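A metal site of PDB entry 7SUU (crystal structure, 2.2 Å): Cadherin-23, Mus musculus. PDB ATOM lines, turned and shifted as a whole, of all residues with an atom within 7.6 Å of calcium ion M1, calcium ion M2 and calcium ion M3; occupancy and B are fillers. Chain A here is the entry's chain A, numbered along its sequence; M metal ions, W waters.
The guanidinium group of Arg 79 lies within salt-bridge range of the side-chain carboxylate of Asp 81 (3.7 Å).
OD1 of Asn 119 lies close to OE1 of Glu 83, at 3.2 Å.
NH1 of Arg 82 sits close to OE2 of Glu 83 (2.9 Å).
The side-chain carboxylate (OD1) of Asp 118 lies close to the side-chain amide oxygen (OD1) of Asn 119 (3.1 Å).
The side-chain carboxylate (OD1) of Asp 115 sits close to the guanidinium group (NE) of Arg 82, at 2.9 Å.
The side-chain carboxylate (OD2) of Asp 115 sits at hydrogen-bond distance from the backbone NH (N) of Glu 159.
The side-chain hydroxyl of Ser 208 sits close to the side-chain carboxylate of Asp 156, at 3.2 Å.
N of Glu 26 sits at hydrogen-bond distance from O of Leu 80 (2.7 Å).
Along chain A the residues within 4 Å of calcium ion M1 span positions 117 to 162.
The nearest printed residue that does not touch calcium ion M1 is Ala 163 (4.3 Å).
Of the 27 residues printed, 7 come within 4 Å of calcium ion M2.
The nearest printed residue that does not touch calcium ion M3 is Arg 82 (4.2 Å).
O of Asn 162 is bound to calcium ion M1 (2.2 Å).
The side-chain carboxylate (OD1) of Asp 117 is bound to calcium ion M1 (2.3 Å).
O of Asn 119 binds calcium ion M1 (2.3 Å).
OD2 of Asp 156 is bound to calcium ion M1 (2.4 Å).
Calcium ion M1 is bound by water W1 (2.4 Å).
Calcium ion M1 is bound by OD2 of Asp 158.
OD1 of Asp 156 is bound to calcium ion M1 (2.5 Å).
Calcium ion M1 has seven donor atoms within binding distance.
Calcium ion M2 is bound by OD1 of Asp 118.
Calcium ion M2 is bound by the side-chain carboxylate (OD1) of Asp 158 (2.3 Å).
Calcium ion M2 is bound by OE2 of Glu 83 (2.3 Å).
Calcium ion M2 is bound by the side-chain carboxylate (OE1) of Glu 25 (2.4 Å).
O of Ile 116 is bound to calcium ion M2 (2.4 Å).
Calcium ion M2 is bound by OD1 of Asp 115 (2.4 Å).
OE1 of Glu 83 is bound to calcium ion M2, 2.8 Å away.
The side-chain carboxylate (OD1) of Asp 81 is bound to calcium ion M3 (2.3 Å).
OE1 of Glu 83 is bound to calcium ion M3, at 2.3 Å.
Calcium ion M3 is bound by OD2 of Asp 118 (2.3 Å).
OE2 of Glu 25 is bound to calcium ion M3 (2.3 Å).
Calcium ion M3 is bound by water W2.
Calcium ion M3 is bound by OE2 of Glu 26 (2.5 Å).
Calcium ion M3 has six donor atoms within binding distance.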
ATOM      1  N   GLU A  25      11.828 -26.743  18.745  1.00  0.00           N
ATOM      2  CA  GLU A  25      11.219 -25.429  19.024  1.00  0.00           C
ATOM      3  C   GLU A  25       9.813 -25.381  18.368  1.00  0.00           C
ATOM      4  O   GLU A  25       9.509 -26.244  17.511  1.00  0.00           O
ATOM      5  CB  GLU A  25      12.147 -24.306  18.541  1.00  0.00           C
ATOM      6  CG  GLU A  25      12.255 -24.219  17.041  1.00  0.00           C
ATOM      7  CD  GLU A  25      12.773 -22.911  16.495  1.00  0.00           C
ATOM      8  OE1 GLU A  25      13.504 -22.986  15.531  1.00  0.00           O
ATOM      9  OE2 GLU A  25      12.406 -21.829  17.019  1.00  0.00           O
ATOM     10  N   GLU A  26       8.987 -24.423  18.784  1.00  0.00           N
ATOM     11  CA  GLU A  26       7.671 -24.061  18.183  1.00  0.00           C
ATOM     12  C   GLU A  26       6.657 -25.217  18.285  1.00  0.00           C
ATOM     13  O   GLU A  26       5.629 -25.169  17.588  1.00  0.00           O
ATOM     14  CB  GLU A  26       7.846 -23.619  16.719  1.00  0.00           C
ATOM     15  CG  GLU A  26       8.807 -22.438  16.530  1.00  0.00           C
ATOM     16  CD  GLU A  26       8.473 -21.109  17.192  1.00  0.00           C
ATOM     17  OE1 GLU A  26       7.422 -21.003  17.857  1.00  0.00           O
ATOM     18  OE2 GLU A  26       9.287 -20.149  17.045  1.00  0.00           O
ATOM     19  N   ARG A  79       4.809 -20.369  24.142  1.00  0.00           N
ATOM     20  CA  ARG A  79       5.553 -20.531  22.889  1.00  0.00           C
ATOM     21  C   ARG A  79       7.011 -20.778  23.256  1.00  0.00           C
ATOM     22  O   ARG A  79       7.519 -20.066  24.130  1.00  0.00           O
ATOM     23  CB  ARG A  79       5.482 -19.264  22.036  1.00  0.00           C
ATOM     24  CG  ARG A  79       6.172 -19.452  20.697  1.00  0.00           C
ATOM     25  CD  ARG A  79       6.088 -18.201  19.858  1.00  0.00           C
ATOM     26  NE  ARG A  79       6.846 -18.392  18.630  1.00  0.00           N
ATOM     27  CZ  ARG A  79       7.209 -17.402  17.817  1.00  0.00           C
ATOM     28  NH1 ARG A  79       7.884 -17.680  16.708  1.00  0.00           N
ATOM     29  NH2 ARG A  79       6.868 -16.172  18.101  1.00  0.00           N
ATOM     30  N   LEU A  80       7.652 -21.737  22.576  1.00  0.00           N
ATOM     31  CA  LEU A  80       9.102 -22.010  22.734  1.00  0.00           C
ATOM     32  C   LEU A  80       9.794 -21.665  21.419  1.00  0.00           C
ATOM     33  O   LEU A  80       9.765 -22.490  20.512  1.00  0.00           O
ATOM     34  CB  LEU A  80       9.302 -23.479  23.135  1.00  0.00           C
ATOM     35  CG  LEU A  80       8.871 -23.825  24.562  1.00  0.00           C
ATOM     36  CD1 LEU A  80       8.866 -25.331  24.766  1.00  0.00           C
ATOM     37  CD2 LEU A  80       9.781 -23.166  25.587  1.00  0.00           C
ATOM     38  N   ASP A  81      10.449 -20.509  21.378  1.00  0.00           N
ATOM     39  CA  ASP A  81      11.110 -19.939  20.184  1.00  0.00           C
ATOM     40  C   ASP A  81      12.619 -19.950  20.426  1.00  0.00           C
ATOM     41  O   ASP A  81      13.061 -19.202  21.315  1.00  0.00           O
ATOM     42  CB  ASP A  81      10.591 -18.522  19.885  1.00  0.00           C
ATOM     43  CG  ASP A  81      11.177 -17.931  18.606  1.00  0.00           C
ATOM     44  OD1 ASP A  81      11.835 -18.658  17.853  1.00  0.00           O
ATOM     45  OD2 ASP A  81      10.981 -16.728  18.396  1.00  0.00           O
ATOM     46  N   ARG A  82      13.363 -20.759  19.657  1.00  0.00           N
ATOM     47  CA  ARG A  82      14.817 -20.952  19.862  1.00  0.00           C
ATOM     48  C   ARG A  82      15.485 -19.619  19.555  1.00  0.00           C
ATOM     49  O   ARG A  82      16.479 -19.326  20.210  1.00  0.00           O
ATOM     50  CB  ARG A  82      15.381 -22.078  18.979  1.00  0.00           C
ATOM     51  CG  ARG A  82      16.869 -22.364  19.160  1.00  0.00           C
ATOM     52  CD  ARG A  82      17.517 -22.964  17.906  1.00  0.00           C
ATOM     53  NE  ARG A  82      17.589 -21.935  16.873  1.00  0.00           N
ATOM     54  CZ  ARG A  82      18.511 -20.980  16.818  1.00  0.00           C
ATOM     55  NH1 ARG A  82      18.449 -20.050  15.885  1.00  0.00           N
ATOM     56  NH2 ARG A  82      19.506 -20.957  17.696  1.00  0.00           N
ATOM     57  N   GLU A  83      14.913 -18.844  18.632  1.00  0.00           N
ATOM     58  CA  GLU A  83      15.431 -17.507  18.243  1.00  0.00           C
ATOM     59  C   GLU A  83      15.162 -16.501  19.360  1.00  0.00           C
ATOM     60  O   GLU A  83      15.816 -15.451  19.360  1.00  0.00           O
ATOM     61  CB  GLU A  83      14.840 -17.054  16.901  1.00  0.00           C
ATOM     62  CG  GLU A  83      15.450 -17.791  15.702  1.00  0.00           C
ATOM     63  CD  GLU A  83      14.896 -19.173  15.357  1.00  0.00           C
ATOM     64  OE1 GLU A  83      13.671 -19.384  15.409  1.00  0.00           O
ATOM     65  OE2 GLU A  83      15.695 -20.048  15.027  1.00  0.00           O
ATOM     66  N   LYS A  84      14.249 -16.789  20.290  1.00  0.00           N
ATOM     67  CA  LYS A  84      14.059 -15.938  21.497  1.00  0.00           C
ATOM     68  C   LYS A  84      15.006 -16.434  22.602  1.00  0.00           C
ATOM     69  O   LYS A  84      15.830 -15.625  23.112  1.00  0.00           O
ATOM     70  CB  LYS A  84      12.615 -15.993  21.988  1.00  0.00           C
ATOM     71  CG  LYS A  84      12.289 -14.971  23.073  1.00  0.00           C
ATOM     72  CD  LYS A  84      10.863 -15.041  23.557  1.00  0.00           C
ATOM     73  CE  LYS A  84      10.620 -14.149  24.756  1.00  0.00           C
ATOM     74  NZ  LYS A  84       9.564 -14.708  25.634  1.00  0.00           N
ATOM     75  N   LEU A 113      16.361 -26.275  22.816  1.00  0.00           N
ATOM     76  CA  LEU A 113      15.454 -26.318  21.647  1.00  0.00           C
ATOM     77  C   LEU A 113      16.284 -26.609  20.407  1.00  0.00           C
ATOM     78  O   LEU A 113      17.226 -25.852  20.144  1.00  0.00           O
ATOM     79  CB  LEU A 113      14.718 -24.993  21.508  1.00  0.00           C
ATOM     80  CG  LEU A 113      13.862 -24.582  22.695  1.00  0.00           C
ATOM     81  CD1 LEU A 113      13.092 -23.303  22.381  1.00  0.00           C
ATOM     82  CD2 LEU A 113      12.923 -25.718  23.099  1.00  0.00           C
ATOM     83  N   GLU A 114      15.948 -27.669  19.687  1.00  0.00           N
ATOM     84  CA  GLU A 114      16.471 -27.990  18.342  1.00  0.00           C
ATOM     85  C   GLU A 114      15.833 -26.988  17.346  1.00  0.00           C
ATOM     86  O   GLU A 114      14.638 -26.726  17.403  1.00  0.00           O
ATOM     87  CB  GLU A 114      16.207 -29.487  18.088  1.00  0.00           C
ATOM     88  CG  GLU A 114      16.200 -29.882  16.605  1.00  0.00           C
ATOM     89  CD  GLU A 114      15.946 -31.349  16.244  1.00  0.00           C
ATOM     90  OE1 GLU A 114      15.908 -31.647  15.028  1.00  0.00           O
ATOM     91  OE2 GLU A 114      15.779 -32.201  17.173  1.00  0.00           O
ATOM     92  N   ASP A 115      16.651 -26.387  16.492  1.00  0.00           N
ATOM     93  CA  ASP A 115      16.225 -25.401  15.468  1.00  0.00           C
ATOM     94  C   ASP A 115      15.302 -26.030  14.417  1.00  0.00           C
ATOM     95  O   ASP A 115      15.577 -27.156  13.952  1.00  0.00           O
ATOM     96  CB  ASP A 115      17.460 -24.834  14.772  1.00  0.00           C
ATOM     97  CG  ASP A 115      17.101 -23.699  13.843  1.00  0.00           C
ATOM     98  OD1 ASP A 115      16.426 -22.692  14.300  1.00  0.00           O
ATOM     99  OD2 ASP A 115      17.514 -23.817  12.694  1.00  0.00           O
ATOM    100  N   ILE A 116      14.250 -25.322  14.015  1.00  0.00           N
ATOM    101  CA  ILE A 116      13.508 -25.631  12.762  1.00  0.00           C
ATOM    102  C   ILE A 116      13.633 -24.418  11.828  1.00  0.00           C
ATOM    103  O   ILE A 116      13.917 -23.296  12.323  1.00  0.00           O
ATOM    104  CB  ILE A 116      12.032 -25.991  13.025  1.00  0.00           C
ATOM    105  CG1 ILE A 116      11.231 -24.751  13.420  1.00  0.00           C
ATOM    106  CG2 ILE A 116      11.909 -27.126  14.047  1.00  0.00           C
ATOM    107  CD1 ILE A 116       9.738 -25.012  13.584  1.00  0.00           C
ATOM    108  N   ASP A 117      13.424 -24.665  10.542  1.00  0.00           N
ATOM    109  CA  ASP A 117      13.604 -23.664   9.474  1.00  0.00           C
ATOM    110  C   ASP A 117      12.369 -22.787   9.448  1.00  0.00           C
ATOM    111  O   ASP A 117      11.541 -23.001   8.564  1.00  0.00           O
ATOM    112  CB  ASP A 117      13.858 -24.316   8.118  1.00  0.00           C
ATOM    113  CG  ASP A 117      14.298 -23.340   7.033  1.00  0.00           C
ATOM    114  OD1 ASP A 117      14.497 -22.112   7.336  1.00  0.00           O
ATOM    115  OD2 ASP A 117      14.480 -23.801   5.908  1.00  0.00           O
ATOM    116  N   ASP A 118      12.221 -21.868  10.398  1.00  0.00           N
ATOM    117  CA  ASP A 118      10.982 -21.043  10.484  1.00  0.00           C
ATOM    118  C   ASP A 118      11.327 -19.572  10.295  1.00  0.00           C
ATOM    119  O   ASP A 118      10.487 -18.750  10.634  1.00  0.00           O
ATOM    120  CB  ASP A 118      10.229 -21.226  11.821  1.00  0.00           C
ATOM    121  CG  ASP A 118      11.082 -20.983  13.065  1.00  0.00           C
ATOM    122  OD1 ASP A 118      12.327 -21.045  12.962  1.00  0.00           O
ATOM    123  OD2 ASP A 118      10.500 -20.754  14.123  1.00  0.00           O
ATOM    124  N   ASN A 119      12.498 -19.257   9.736  1.00  0.00           N
ATOM    125  CA  ASN A 119      12.873 -17.859   9.408  1.00  0.00           C
ATOM    126  C   ASN A 119      13.436 -17.827   7.998  1.00  0.00           C
ATOM    127  O   ASN A 119      14.021 -18.822   7.568  1.00  0.00           O
ATOM    128  CB  ASN A 119      13.867 -17.293  10.420  1.00  0.00           C
ATOM    129  CG  ASN A 119      13.224 -17.120  11.783  1.00  0.00           C
ATOM    130  OD1 ASN A 119      13.104 -18.073  12.557  1.00  0.00           O
ATOM    131  ND2 ASN A 119      12.778 -15.910  12.070  1.00  0.00           N
ATOM    132  N   GLU A 120      13.332 -16.695   7.333  1.00  0.00           N
ATOM    133  CA  GLU A 120      13.930 -16.524   5.988  1.00  0.00           C
ATOM    134  C   GLU A 120      14.943 -15.394   6.084  1.00  0.00           C
ATOM    135  O   GLU A 120      14.872 -14.558   6.998  1.00  0.00           O
ATOM    136  CB  GLU A 120      12.868 -16.245   4.934  1.00  0.00           C
ATOM    137  CG  GLU A 120      12.112 -14.961   5.168  1.00  0.00           C
ATOM    138  CD  GLU A 120      10.924 -14.728   4.233  1.00  0.00           C
ATOM    139  OE1 GLU A 120      10.293 -13.658   4.344  1.00  0.00           O
ATOM    140  OE2 GLU A 120      10.648 -15.605   3.388  1.00  0.00           O
ATOM    141  N   PRO A 121      15.905 -15.330   5.114  1.00  0.00           N
ATOM    142  CA  PRO A 121      16.805 -14.186   4.994  1.00  0.00           C
ATOM    143  C   PRO A 121      16.036 -12.870   4.886  1.00  0.00           C
ATOM    144  O   PRO A 121      15.155 -12.772   4.057  1.00  0.00           O
ATOM    145  CB  PRO A 121      17.584 -14.485   3.715  1.00  0.00           C
ATOM    146  CG  PRO A 121      17.555 -15.962   3.599  1.00  0.00           C
ATOM    147  CD  PRO A 121      16.182 -16.378   4.116  1.00  0.00           C
ATOM    148  N   ASP A 156      19.610 -14.839   8.176  1.00  0.00           N
ATOM    149  CA  ASP A 156      18.584 -15.857   8.508  1.00  0.00           C
ATOM    150  C   ASP A 156      18.795 -16.252   9.973  1.00  0.00           C
ATOM    151  O   ASP A 156      19.889 -16.754  10.306  1.00  0.00           O
ATOM    152  CB  ASP A 156      18.681 -17.039   7.545  1.00  0.00           C
ATOM    153  CG  ASP A 156      17.579 -18.080   7.606  1.00  0.00           C
ATOM    154  OD1 ASP A 156      17.247 -18.549   8.700  1.00  0.00           O
ATOM    155  OD2 ASP A 156      17.126 -18.499   6.525  1.00  0.00           O
ATOM    156  N   ALA A 157      17.769 -16.091  10.800  1.00  0.00           N
ATOM    157  CA  ALA A 157      17.856 -16.230  12.279  1.00  0.00           C
ATOM    158  C   ALA A 157      17.942 -17.708  12.682  1.00  0.00           C
ATOM    159  O   ALA A 157      18.134 -17.982  13.880  1.00  0.00           O
ATOM    160  CB  ALA A 157      16.700 -15.511  12.953  1.00  0.00           C
ATOM    161  N   ASP A 158      17.825 -18.627  11.722  1.00  0.00           N
ATOM    162  CA  ASP A 158      17.836 -20.092  12.000  1.00  0.00           C
ATOM    163  C   ASP A 158      19.290 -20.548  12.182  1.00  0.00           C
ATOM    164  O   ASP A 158      20.131 -19.703  12.401  1.00  0.00           O
ATOM    165  CB  ASP A 158      17.069 -20.861  10.923  1.00  0.00           C
ATOM    166  CG  ASP A 158      15.574 -20.584  10.907  1.00  0.00           C
ATOM    167  OD1 ASP A 158      14.980 -20.359  11.986  1.00  0.00           O
ATOM    168  OD2 ASP A 158      15.026 -20.546   9.834  1.00  0.00           O
ATOM    169  N   GLU A 159      19.558 -21.848  12.115  1.00  0.00           N
ATOM    170  CA  GLU A 159      20.876 -22.451  12.476  1.00  0.00           C
ATOM    171  C   GLU A 159      21.418 -23.319  11.332  1.00  0.00           C
ATOM    172  O   GLU A 159      20.658 -24.077  10.721  1.00  0.00           O
ATOM    173  CB  GLU A 159      20.689 -23.302  13.730  1.00  0.00           C
ATOM    174  CG  GLU A 159      21.958 -23.565  14.477  1.00  0.00           C
ATOM    175  CD  GLU A 159      22.359 -22.449  15.410  1.00  0.00           C
ATOM    176  OE1 GLU A 159      22.302 -21.247  15.007  1.00  0.00           O
ATOM    177  OE2 GLU A 159      22.716 -22.778  16.547  1.00  0.00           O
ATOM    178  N   GLY A 160      22.719 -23.224  11.078  1.00  0.00           N
ATOM    179  CA  GLY A 160      23.430 -24.129  10.144  1.00  0.00           C
ATOM    180  C   GLY A 160      22.673 -24.210   8.819  1.00  0.00           C
ATOM    181  O   GLY A 160      22.395 -23.179   8.203  1.00  0.00           O
ATOM    182  N   PRO A 161      22.299 -25.423   8.351  1.00  0.00           N
ATOM    183  CA  PRO A 161      21.713 -25.571   7.017  1.00  0.00           C
ATOM    184  C   PRO A 161      20.305 -24.975   6.860  1.00  0.00           C
ATOM    185  O   PRO A 161      19.804 -24.962   5.761  1.00  0.00           O
ATOM    186  CB  PRO A 161      21.732 -27.086   6.746  1.00  0.00           C
ATOM    187  CG  PRO A 161      21.886 -27.735   8.125  1.00  0.00           C
ATOM    188  CD  PRO A 161      22.546 -26.706   9.032  1.00  0.00           C
ATOM    189  N   ASN A 162      19.717 -24.461   7.937  1.00  0.00           N
ATOM    190  CA  ASN A 162      18.420 -23.747   7.921  1.00  0.00           C
ATOM    191  C   ASN A 162      18.648 -22.249   7.697  1.00  0.00           C
ATOM    192  O   ASN A 162      17.653 -21.530   7.527  1.00  0.00           O
ATOM    193  CB  ASN A 162      17.643 -23.953   9.221  1.00  0.00           C
ATOM    194  CG  ASN A 162      17.321 -25.404   9.488  1.00  0.00           C
ATOM    195  OD1 ASN A 162      17.072 -26.157   8.559  1.00  0.00           O
ATOM    196  ND2 ASN A 162      17.315 -25.791  10.759  1.00  0.00           N
ATOM    197  N   ALA A 163      19.901 -21.792   7.661  1.00  0.00           N
ATOM    198  CA  ALA A 163      20.252 -20.358   7.671  1.00  0.00           C
ATOM    199  C   ALA A 163      21.134 -20.011   6.467  1.00  0.00           C
ATOM    200  O   ALA A 163      21.900 -19.047   6.573  1.00  0.00           O
ATOM    201  CB  ALA A 163      20.957 -20.025   8.961  1.00  0.00           C
ATOM    202  N   ILE A 164      21.028 -20.744   5.351  1.00  0.00           N
ATOM    203  CA  ILE A 164      21.844 -20.425   4.142  1.00  0.00           C
ATOM    204  C   ILE A 164      21.286 -19.165   3.506  1.00  0.00           C
ATOM    205  O   ILE A 164      20.091 -19.109   3.295  1.00  0.00           O
ATOM    206  CB  ILE A 164      21.871 -21.605   3.168  1.00  0.00           C
ATOM    207  CG1 ILE A 164      22.529 -22.817   3.836  1.00  0.00           C
ATOM    208  CG2 ILE A 164      22.580 -21.164   1.886  1.00  0.00           C
ATOM    209  CD1 ILE A 164      22.282 -24.146   3.155  1.00  0.00           C
ATOM    210  N   SER A 208      17.035 -18.390   0.700  1.00  0.00           N
ATOM    211  CA  SER A 208      17.679 -19.683   1.027  1.00  0.00           C
ATOM    212  C   SER A 208      17.555 -20.623  -0.162  1.00  0.00           C
ATOM    213  O   SER A 208      18.218 -21.665  -0.146  1.00  0.00           O
ATOM    214  CB  SER A 208      17.122 -20.279   2.307  1.00  0.00           C
ATOM    215  OG  SER A 208      17.399 -19.405   3.417  1.00  0.00           O
HETATM  216 CA    CA M   1      15.831 -20.264   7.513  1.00  0.00          CA
HETATM  217 CA    CA M   2      14.387 -21.563  13.865  1.00  0.00          CA
HETATM  218 CA    CA M   3      11.547 -19.925  16.002  1.00  0.00          CA
HETATM  219  O   HOH W   1      15.775 -20.490   5.094  1.00  0.00           O
HETATM  220  O   HOH W   2      11.056 -17.838  14.807  1.00  0.00           O
